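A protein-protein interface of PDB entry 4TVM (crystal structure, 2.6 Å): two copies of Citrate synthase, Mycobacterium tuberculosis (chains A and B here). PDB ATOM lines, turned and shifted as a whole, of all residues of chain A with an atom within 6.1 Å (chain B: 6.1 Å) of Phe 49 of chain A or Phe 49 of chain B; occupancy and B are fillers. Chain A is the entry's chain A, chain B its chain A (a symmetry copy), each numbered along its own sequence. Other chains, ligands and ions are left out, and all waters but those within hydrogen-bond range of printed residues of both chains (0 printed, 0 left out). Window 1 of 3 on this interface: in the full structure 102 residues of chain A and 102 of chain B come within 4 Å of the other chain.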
ATOM      1  N   ASP A  46      -0.689  12.311   3.569  1.00  0.00           N
ATOM      2  CA  ASP A  46      -1.292  11.703   2.370  1.00  0.00           C
ATOM      3  C   ASP A  46      -0.876  12.410   1.104  1.00  0.00           C
ATOM      4  O   ASP A  46      -1.480  13.400   0.719  1.00  0.00           O
ATOM      5  CB  ASP A  46      -2.817  11.777   2.458  1.00  0.00           C
ATOM      6  CG  ASP A  46      -3.511  10.958   1.376  1.00  0.00           C
ATOM      7  OD1 ASP A  46      -2.872  10.101   0.724  1.00  0.00           O
ATOM      8  OD2 ASP A  46      -4.718  11.158   1.199  1.00  0.00           O
ATOM      9  N   VAL A  47       0.149  11.897   0.449  1.00  0.00           N
ATOM     10  CA  VAL A  47       0.636  12.490  -0.795  1.00  0.00           C
ATOM     11  C   VAL A  47      -0.487  12.734  -1.806  1.00  0.00           C
ATOM     12  O   VAL A  47      -1.279  11.852  -2.088  1.00  0.00           O
ATOM     13  CB  VAL A  47       1.673  11.584  -1.469  1.00  0.00           C
ATOM     14  CG1 VAL A  47       2.201  12.231  -2.755  1.00  0.00           C
ATOM     15  CG2 VAL A  47       2.806  11.256  -0.491  1.00  0.00           C
ATOM     16  N   GLY A  48      -0.560  13.953  -2.312  1.00  0.00           N
ATOM     17  CA  GLY A  48      -1.547  14.340  -3.302  1.00  0.00           C
ATOM     18  C   GLY A  48      -2.953  14.573  -2.767  1.00  0.00           C
ATOM     19  O   GLY A  48      -3.855  14.917  -3.544  1.00  0.00           O
ATOM     20  N   PHE A  49      -3.155  14.396  -1.462  1.00  0.00           N
ATOM     21  CA  PHE A  49      -4.512  14.347  -0.878  1.00  0.00           C
ATOM     22  C   PHE A  49      -5.361  13.197  -1.437  1.00  0.00           C
ATOM     23  O   PHE A  49      -6.589  13.240  -1.397  1.00  0.00           O
ATOM     24  CB  PHE A  49      -5.249  15.666  -1.095  1.00  0.00           C
ATOM     25  CG  PHE A  49      -4.597  16.844  -0.443  1.00  0.00           C
ATOM     26  CD1 PHE A  49      -4.457  16.895   0.938  1.00  0.00           C
ATOM     27  CD2 PHE A  49      -4.140  17.927  -1.203  1.00  0.00           C
ATOM     28  CE1 PHE A  49      -3.861  17.997   1.548  1.00  0.00           C
ATOM     29  CE2 PHE A  49      -3.544  19.015  -0.603  1.00  0.00           C
ATOM     30  CZ  PHE A  49      -3.397  19.050   0.780  1.00  0.00           C
ATOM     31  N   ALA A  50      -4.711  12.153  -1.933  1.00  0.00           N
ATOM     32  CA  ALA A  50      -5.407  11.147  -2.742  1.00  0.00           C
ATOM     33  C   ALA A  50      -6.506  10.472  -1.968  1.00  0.00           C
ATOM     34  O   ALA A  50      -7.529  10.091  -2.557  1.00  0.00           O
ATOM     35  CB  ALA A  50      -4.429  10.116  -3.288  1.00  0.00           C
ATOM     36  N   ASN A  51      -6.308  10.341  -0.649  1.00  0.00           N
ATOM     37  CA  ASN A  51      -7.270   9.657   0.225  1.00  0.00           C
ATOM     38  C   ASN A  51      -7.995  10.537   1.194  1.00  0.00           C
ATOM     39  O   ASN A  51      -8.745  10.051   2.041  1.00  0.00           O
ATOM     40  CB  ASN A  51      -6.582   8.529   0.959  1.00  0.00           C
ATOM     41  CG  ASN A  51      -6.137   7.441   0.012  1.00  0.00           C
ATOM     42  OD1 ASN A  51      -6.973   6.717  -0.521  1.00  0.00           O
ATOM     43  ND2 ASN A  51      -4.827   7.348  -0.243  1.00  0.00           N
ATOM     44  N   THR A  52      -7.811  11.839   1.042  1.00  0.00           N
ATOM     45  CA  THR A  52      -8.442  12.807   1.913  1.00  0.00           C
ATOM     46  C   THR A  52      -9.471  13.570   1.138  1.00  0.00           C
ATOM     47  O   THR A  52      -9.204  13.979   0.004  1.00  0.00           O
ATOM     48  CB  THR A  52      -7.417  13.820   2.417  1.00  0.00           C
ATOM     49  OG1 THR A  52      -6.314  13.135   3.038  1.00  0.00           O
ATOM     50  CG2 THR A  52      -8.064  14.799   3.395  1.00  0.00           C
ATOM     51  N   ALA A  53     -10.618  13.794   1.779  1.00  0.00           N
ATOM     52  CA  ALA A  53     -11.684  14.626   1.245  1.00  0.00           C
ATOM     53  C   ALA A  53     -11.910  15.798   2.162  1.00  0.00           C
ATOM     54  O   ALA A  53     -12.092  15.605   3.360  1.00  0.00           O
ATOM     55  CB  ALA A  53     -12.960  13.828   1.177  1.00  0.00           C
ATOM     56  N   ALA A  54     -11.951  17.009   1.618  1.00  0.00           N
ATOM     57  CA  ALA A  54     -12.234  18.177   2.459  1.00  0.00           C
ATOM     58  C   ALA A  54     -13.635  18.751   2.239  1.00  0.00           C
ATOM     59  O   ALA A  54     -14.055  19.672   2.939  1.00  0.00           O
ATOM     60  CB  ALA A  54     -11.195  19.253   2.233  1.00  0.00           C
ATOM     61  N   SER A 239     -10.086  21.762  -7.294  1.00  0.00           N
ATOM     62  CA  SER A 239      -9.728  21.887  -5.899  1.00  0.00           C
ATOM     63  C   SER A 239      -8.978  23.181  -5.766  1.00  0.00           C
ATOM     64  O   SER A 239      -8.902  23.699  -4.695  1.00  0.00           O
ATOM     65  CB  SER A 239      -8.867  20.749  -5.408  1.00  0.00           C
ATOM     66  OG  SER A 239      -9.661  19.599  -5.203  1.00  0.00           O
ATOM     67  N   LEU A 243      -9.858  26.239  -3.281  1.00  0.00           N
ATOM     68  CA  LEU A 243      -8.901  26.799  -2.342  1.00  0.00           C
ATOM     69  C   LEU A 243      -8.831  28.342  -2.368  1.00  0.00           C
ATOM     70  O   LEU A 243      -8.834  29.011  -1.339  1.00  0.00           O
ATOM     71  CB  LEU A 243      -7.540  26.198  -2.680  1.00  0.00           C
ATOM     72  CG  LEU A 243      -6.438  26.101  -1.594  1.00  0.00           C
ATOM     73  CD1 LEU A 243      -6.926  25.536  -0.273  1.00  0.00           C
ATOM     74  CD2 LEU A 243      -5.289  25.255  -2.092  1.00  0.00           C
ATOM     75  N   GLY A 411      -8.713  27.285   3.844  1.00  0.00           N
ATOM     76  CA  GLY A 411      -7.817  26.139   3.712  1.00  0.00           C
ATOM     77  C   GLY A 411      -6.466  26.323   4.380  1.00  0.00           C
ATOM     78  O   GLY A 411      -5.676  27.160   3.979  1.00  0.00           O
ATOM     79  N   ARG A 412      -6.196  25.490   5.375  1.00  0.00           N
ATOM     80  CA  ARG A 412      -5.005  25.588   6.219  1.00  0.00           C
ATOM     81  C   ARG A 412      -4.378  24.196   6.351  1.00  0.00           C
ATOM     82  O   ARG A 412      -4.511  23.551   7.379  1.00  0.00           O
ATOM     83  CB  ARG A 412      -5.425  26.096   7.601  1.00  0.00           C
ATOM     84  CG  ARG A 412      -4.301  26.668   8.444  1.00  0.00           C
ATOM     85  CD  ARG A 412      -4.119  28.152   8.142  1.00  0.00           C
ATOM     86  NE  ARG A 412      -2.805  28.673   8.531  1.00  0.00           N
ATOM     87  CZ  ARG A 412      -1.664  28.376   7.913  1.00  0.00           C
ATOM     88  NH1 ARG A 412      -1.660  27.529   6.882  1.00  0.00           N
ATOM     89  NH2 ARG A 412      -0.518  28.908   8.334  1.00  0.00           N
ATOM     90  N   PRO A 413      -3.728  23.704   5.297  1.00  0.00           N
ATOM     91  CA  PRO A 413      -3.135  22.362   5.414  1.00  0.00           C
ATOM     92  C   PRO A 413      -1.905  22.312   6.304  1.00  0.00           C
ATOM     93  O   PRO A 413      -1.421  23.352   6.746  1.00  0.00           O
ATOM     94  CB  PRO A 413      -2.736  22.018   3.977  1.00  0.00           C
ATOM     95  CG  PRO A 413      -3.501  22.967   3.116  1.00  0.00           C
ATOM     96  CD  PRO A 413      -3.660  24.220   3.922  1.00  0.00           C
ATOM     97  N   ARG A 414      -1.400  21.102   6.519  1.00  0.00           N
ATOM     98  CA  ARG A 414      -0.246  20.895   7.337  1.00  0.00           C
ATOM     99  C   ARG A 414       0.976  20.471   6.531  1.00  0.00           C
ATOM    100  O   ARG A 414       0.947  20.429   5.281  1.00  0.00           O
ATOM    101  CB  ARG A 414      -0.579  19.859   8.417  1.00  0.00           C
ATOM    102  CG  ARG A 414      -1.692  20.315   9.336  1.00  0.00           C
ATOM    103  CD  ARG A 414      -1.315  21.620  10.012  1.00  0.00           C
ATOM    104  NE  ARG A 414      -2.384  22.096  10.884  1.00  0.00           N
ATOM    105  CZ  ARG A 414      -2.255  23.076  11.778  1.00  0.00           C
ATOM    106  NH1 ARG A 414      -1.086  23.707  11.932  1.00  0.00           N
ATOM    107  NH2 ARG A 414      -3.300  23.427  12.521  1.00  0.00           N
ATOM    108  N   ASP B  46     -11.805  16.038   6.313  1.00  0.00           N
ATOM    109  CA  ASP B  46     -11.152  17.079   7.126  1.00  0.00           C
ATOM    110  C   ASP B  46     -11.328  18.456   6.534  1.00  0.00           C
ATOM    111  O   ASP B  46     -10.564  18.863   5.672  1.00  0.00           O
ATOM    112  CB  ASP B  46      -9.650  16.807   7.215  1.00  0.00           C
ATOM    113  CG  ASP B  46      -8.947  17.699   8.232  1.00  0.00           C
ATOM    114  OD1 ASP B  46      -9.612  18.333   9.082  1.00  0.00           O
ATOM    115  OD2 ASP B  46      -7.713  17.741   8.193  1.00  0.00           O
ATOM    116  N   VAL B  47     -12.329  19.178   7.001  1.00  0.00           N
ATOM    117  CA  VAL B  47     -12.593  20.529   6.512  1.00  0.00           C
ATOM    118  C   VAL B  47     -11.341  21.409   6.519  1.00  0.00           C
ATOM    119  O   VAL B  47     -10.641  21.494   7.513  1.00  0.00           O
ATOM    120  CB  VAL B  47     -13.653  21.230   7.369  1.00  0.00           C
ATOM    121  CG1 VAL B  47     -13.947  22.634   6.825  1.00  0.00           C
ATOM    122  CG2 VAL B  47     -14.923  20.375   7.446  1.00  0.00           C
ATOM    123  N   GLY B  48     -11.057  22.028   5.386  1.00  0.00           N
ATOM    124  CA  GLY B  48      -9.922  22.919   5.235  1.00  0.00           C
ATOM    125  C   GLY B  48      -8.568  22.237   5.101  1.00  0.00           C
ATOM    126  O   GLY B  48      -7.547  22.925   4.957  1.00  0.00           O
ATOM    127  N   PHE B  49      -8.540  20.906   5.141  1.00  0.00           N
ATOM    128  CA  PHE B  49      -7.275  20.153   5.273  1.00  0.00           C
ATOM    129  C   PHE B  49      -6.521  20.475   6.571  1.00  0.00           C
ATOM    130  O   PHE B  49      -5.310  20.284   6.663  1.00  0.00           O
ATOM    131  CB  PHE B  49      -6.356  20.412   4.082  1.00  0.00           C
ATOM    132  CG  PHE B  49      -6.923  19.976   2.768  1.00  0.00           C
ATOM    133  CD1 PHE B  49      -7.211  18.638   2.536  1.00  0.00           C
ATOM    134  CD2 PHE B  49      -7.150  20.898   1.739  1.00  0.00           C
ATOM    135  CE1 PHE B  49      -7.727  18.228   1.308  1.00  0.00           C
ATOM    136  CE2 PHE B  49      -7.667  20.497   0.527  1.00  0.00           C
ATOM    137  CZ  PHE B  49      -7.964  19.156   0.310  1.00  0.00           C
ATOM    138  N   ALA B  50      -7.238  20.936   7.586  1.00  0.00           N
ATOM    139  CA  ALA B  50      -6.588  21.540   8.755  1.00  0.00           C
ATOM    140  C   ALA B  50      -5.679  20.565   9.453  1.00  0.00           C
ATOM    141  O   ALA B  50      -4.653  20.976  10.015  1.00  0.00           O
ATOM    142  CB  ALA B  50      -7.622  22.094   9.727  1.00  0.00           C
ATOM    143  N   ASN B  51      -6.040  19.276   9.401  1.00  0.00           N
ATOM    144  CA  ASN B  51      -5.279  18.220  10.079  1.00  0.00           C
ATOM    145  C   ASN B  51      -4.561  17.264   9.177  1.00  0.00           C
ATOM    146  O   ASN B  51      -3.980  16.282   9.640  1.00  0.00           O
ATOM    147  CB  ASN B  51      -6.183  17.463  11.026  1.00  0.00           C
ATOM    148  CG  ASN B  51      -6.652  18.339  12.162  1.00  0.00           C
ATOM    149  OD1 ASN B  51      -5.860  18.682  13.034  1.00  0.00           O
ATOM    150  ND2 ASN B  51      -7.926  18.748  12.136  1.00  0.00           N
ATOM    151  N   THR B  52      -4.561  17.575   7.890  1.00  0.00           N
ATOM    152  CA  THR B  52      -3.915  16.739   6.903  1.00  0.00           C
ATOM    153  C   THR B  52      -2.715  17.452   6.360  1.00  0.00           C
ATOM    154  O   THR B  52      -2.798  18.647   6.063  1.00  0.00           O
ATOM    155  CB  THR B  52      -4.853  16.478   5.727  1.00  0.00           C
ATOM    156  OG1 THR B  52      -6.096  15.933   6.202  1.00  0.00           O
ATOM    157  CG2 THR B  52      -4.202  15.534   4.717  1.00  0.00           C
ATOM    158  N   ALA B  53      -1.629  16.698   6.192  1.00  0.00           N
ATOM    159  CA  ALA B  53      -0.413  17.177   5.557  1.00  0.00           C
ATOM    160  C   ALA B  53      -0.146  16.368   4.316  1.00  0.00           C
ATOM    161  O   ALA B  53      -0.126  15.142   4.383  1.00  0.00           O
ATOM    162  CB  ALA B  53       0.751  16.997   6.496  1.00  0.00           C
ATOM    163  N   ALA B  54       0.111  17.026   3.191  1.00  0.00           N
ATOM    164  CA  ALA B  54       0.443  16.285   1.971  1.00  0.00           C
ATOM    165  C   ALA B  54       1.921  16.384   1.590  1.00  0.00           C
ATOM    166  O   ALA B  54       2.373  15.737   0.645  1.00  0.00           O
ATOM    167  CB  ALA B  54      -0.419  16.753   0.819  1.00  0.00           C
ATOM    168  N   SER B 239      -0.113  26.555  -0.637  1.00  0.00           N
ATOM    169  CA  SER B 239      -0.607  25.237  -0.969  1.00  0.00           C
ATOM    170  C   SER B 239      -1.197  25.338  -2.345  1.00  0.00           C
ATOM    171  O   SER B 239      -1.328  24.346  -2.993  1.00  0.00           O
ATOM    172  CB  SER B 239      -1.656  24.742  -0.003  1.00  0.00           C
ATOM    173  OG  SER B 239      -1.044  24.318   1.197  1.00  0.00           O
ATOM    174  N   LEU B 243      -0.223  23.098  -5.561  1.00  0.00           N
ATOM    175  CA  LEU B 243      -1.202  22.353  -6.334  1.00  0.00           C
ATOM    176  C   LEU B 243      -1.072  22.550  -7.860  1.00  0.00           C
ATOM    177  O   LEU B 243      -1.100  21.605  -8.643  1.00  0.00           O
ATOM    178  CB  LEU B 243      -2.581  22.796  -5.855  1.00  0.00           C
ATOM    179  CG  LEU B 243      -3.802  21.855  -6.014  1.00  0.00           C
ATOM    180  CD1 LEU B 243      -3.543  20.430  -5.561  1.00  0.00           C
ATOM    181  CD2 LEU B 243      -4.985  22.403  -5.251  1.00  0.00           C
ATOM    182  N   GLY B 411      -2.027  16.326  -7.578  1.00  0.00           N
ATOM    183  CA  GLY B 411      -3.040  16.450  -6.533  1.00  0.00           C
ATOM    184  C   GLY B 411      -4.423  15.982  -6.948  1.00  0.00           C
ATOM    185  O   GLY B 411      -5.050  16.566  -7.815  1.00  0.00           O
ATOM    186  N   ARG B 412      -4.908  14.948  -6.276  1.00  0.00           N
ATOM    187  CA  ARG B 412      -6.165  14.277  -6.609  1.00  0.00           C
ATOM    188  C   ARG B 412      -6.975  14.080  -5.324  1.00  0.00           C
ATOM    189  O   ARG B 412      -7.042  12.980  -4.796  1.00  0.00           O
ATOM    190  CB  ARG B 412      -5.843  12.914  -7.229  1.00  0.00           C
ATOM    191  CG  ARG B 412      -6.974  12.285  -8.022  1.00  0.00           C
ATOM    192  CD  ARG B 412      -6.930  12.764  -9.470  1.00  0.00           C
ATOM    193  NE  ARG B 412      -8.203  12.601 -10.180  1.00  0.00           N
ATOM    194  CZ  ARG B 412      -9.295  13.325  -9.942  1.00  0.00           C
ATOM    195  NH1 ARG B 412      -9.289  14.252  -8.983  1.00  0.00           N
ATOM    196  NH2 ARG B 412     -10.405  13.111 -10.647  1.00  0.00           N
ATOM    197  N   PRO B 413      -7.558  15.149  -4.786  1.00  0.00           N
ATOM    198  CA  PRO B 413      -8.326  14.968  -3.544  1.00  0.00           C
ATOM    199  C   PRO B 413      -9.646  14.241  -3.740  1.00  0.00           C
ATOM    200  O   PRO B 413     -10.040  13.976  -4.874  1.00  0.00           O
ATOM    201  CB  PRO B 413      -8.600  16.400  -3.077  1.00  0.00           C
ATOM    202  CG  PRO B 413      -7.629  17.252  -3.822  1.00  0.00           C
ATOM    203  CD  PRO B 413      -7.404  16.568  -5.137  1.00  0.00           C
ATOM    204  N   ARG B 414     -10.322  13.966  -2.630  1.00  0.00           N
ATOM    205  CA  ARG B 414     -11.578  13.283  -2.655  1.00  0.00           C
ATOM    206  C   ARG B 414     -12.744  14.190  -2.279  1.00  0.00           C
ATOM    207  O   ARG B 414     -12.579  15.414  -2.084  1.00  0.00           O
ATOM    208  CB  ARG B 414     -11.504  12.067  -1.725  1.00  0.00           C
ATOM    209  CG  ARG B 414     -10.454  11.067  -2.159  1.00  0.00           C
ATOM    210  CD  ARG B 414     -10.735  10.586  -3.570  1.00  0.00           C
ATOM    211  NE  ARG B 414      -9.721   9.640  -4.023  1.00  0.00           N
ATOM    212  CZ  ARG B 414      -9.825   8.878  -5.111  1.00  0.00           C
ATOM    213  NH1 ARG B 414     -10.914   8.941  -5.885  1.00  0.00           N
ATOM    214  NH2 ARG B 414      -8.834   8.050  -5.429  1.00  0.00           N
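Printed residues of chain B within 4 Å of Gly 48 of chain A: Gly 411, Arg 412 and Pro 413. Printed residues of chain A within 4 Å of Thr 52 of chain B: Thr 52 (3.6 Å), Pro 413 (3.8 Å) and Arg 414 (2.9 Å). Asn 51 of chain B touches none of the printed residues of chain A. Leu 243 of chain B touches none of the printed residues of chain A. The nearest printed residue of chain B that does not touch Phe 49 of chain A is Thr 52 of chain B (4.02 Å). The nearest printed residue of chain A that does not touch Phe 49 of chain B is Thr 52 of chain A (4.03 Å). The nearest printed residue of chain A that does not touch Ala 54 of chain B is Arg 414 of chain A (4.1 Å).
O of Gly 48 of chain A touches N of Pro 413 of chain B, 3.9 Å away. Phe 49 of chain A touches Pro 413 of chain B. Phe 49 of chain A touches Arg 414 of chain B (O to N, 3.998 Å). Thr 52 of chain A touches Thr 52 of chain B (OG1 to CG2, 3.6 Å). Pro 413 of chain B touches Thr 52 of chain A. CB of Ala 54 of chain A touches O of Asp 46 of chain B, 3.5 Å away. CE1 of Phe 49 of chain B touches CB of Ala 54 of chain A, 3.7 Å away. CG of Pro 413 of chain B touches OG of Ser 239 of chain A (3.4 Å). Gly 48 of chain B touches Pro 413 of chain A. Arg 414 of chain A touches Ala 53 of chain B (C to CB, 3.5 Å).
Asp 46 of chain A touches Ala 54 of chain B, and with the chains exchanged Ala 54 of chain A touches Asp 46 of chain B. Gly 48 of chain A touches Arg 412 of chain B, and with the chains exchanged Arg 412 of chain A touches Gly 48 of chain B. Gly 48 of chain A touches Pro 413 of chain B, and with the chains exchanged Pro 413 of chain A touches Gly 48 of chain B. Thr 52 of chain B touches its own counterpart, Thr 52 of chain A. Positions printed for both chains: 46, 47, 48, 49, 50, 51, 52, 53, 54, 239, 243, 411, 412, 413 and 414.
O of Ala 53 of chain A lies within hydrogen-bond range of N of Asp 46 of chain B, at 3.0 Å. O of Gly 48 of chain A lies within hydrogen-bond range of N of Arg 412 of chain B (2.9 Å). N of Arg 414 of chain A sits at hydrogen-bond distance from O of Thr 52 of chain B, 2.9 Å away. The backbone carbonyl oxygen of Phe 49 of chain B sits close to the backbone carbonyl oxygen of Arg 412 of chain A, 3.4 Å away. The guanidinium group (NE) of Arg 414 of chain A is in hydrogen-bond range of the backbone carbonyl oxygen (O) of Ala 50 of chain B, 2.7 Å away. The backbone NH of Arg 412 of chain A sits at hydrogen-bond distance from the backbone carbonyl oxygen of Gly 48 of chain B (2.9 Å). The backbone NH of Asp 46 of chain A lies within hydrogen-bond range of the backbone carbonyl oxygen of Ala 53 of chain B (3.0 Å). The backbone carbonyl oxygen (O) of Phe 49 of chain A sits close to the backbone carbonyl oxygen (O) of Arg 412 of chain B (3.4 Å). NE of Arg 414 of chain B is in hydrogen-bond range of O of Ala 50 of chain A, 2.7 Å away. The backbone carbonyl oxygen (O) of Thr 52 of chain A is in hydrogen-bond range of the backbone NH (N) of Arg 414 of chain B (2.9 Å).
Of the 15 printed residues of chain B, 13 touch a printed residue of chain A. Printed residues of chain B that touch a printed residue of chain A: Asp 46, Val 47, Gly 48, Phe 49, Ala 50, Thr 52, Ala 53, Ala 54, Ser 239, Gly 411, Arg 412, Pro 413 and Arg 414. Hydrophobic or aromatic side chains of chain B that line the printed part of chain A: Phe 49, Ala 53, Ala 54 and Pro 413. Hydrophobic or aromatic side chains of chain A within 4 Å of the printed part of chain B: Phe 49, Ala 53, Ala 54 and Pro 413. Among the printed residues, no Asp or Glu carboxylate lies within 4 Å of a Lys or Arg side-chain nitrogen of the other chain.
OD2 of Asp 46 of chain A is in hydrogen-bond range of N of Ala 50 of chain A, 3.3 Å away. OD2 of Asp 46 of chain A lies within hydrogen-bond range of OG1 of Thr 52 of chain A. OD2 of Asp 46 of chain A sits at hydrogen-bond distance from N of Asn 51 of chain A, 2.6 Å away. The side-chain carboxylate (OD2) of Asp 46 of chain B is in hydrogen-bond range of the side-chain hydroxyl (OG1) of Thr 52 of chain B (3.1 Å). The side-chain carboxylate (OD2) of Asp 46 of chain B is in hydrogen-bond range of the backbone NH (N) of Asn 51 of chain B, at 2.6 Å. OD2 of Asp 46 of chain B is in hydrogen-bond range of N of Ala 50 of chain B, 3.3 Å away.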
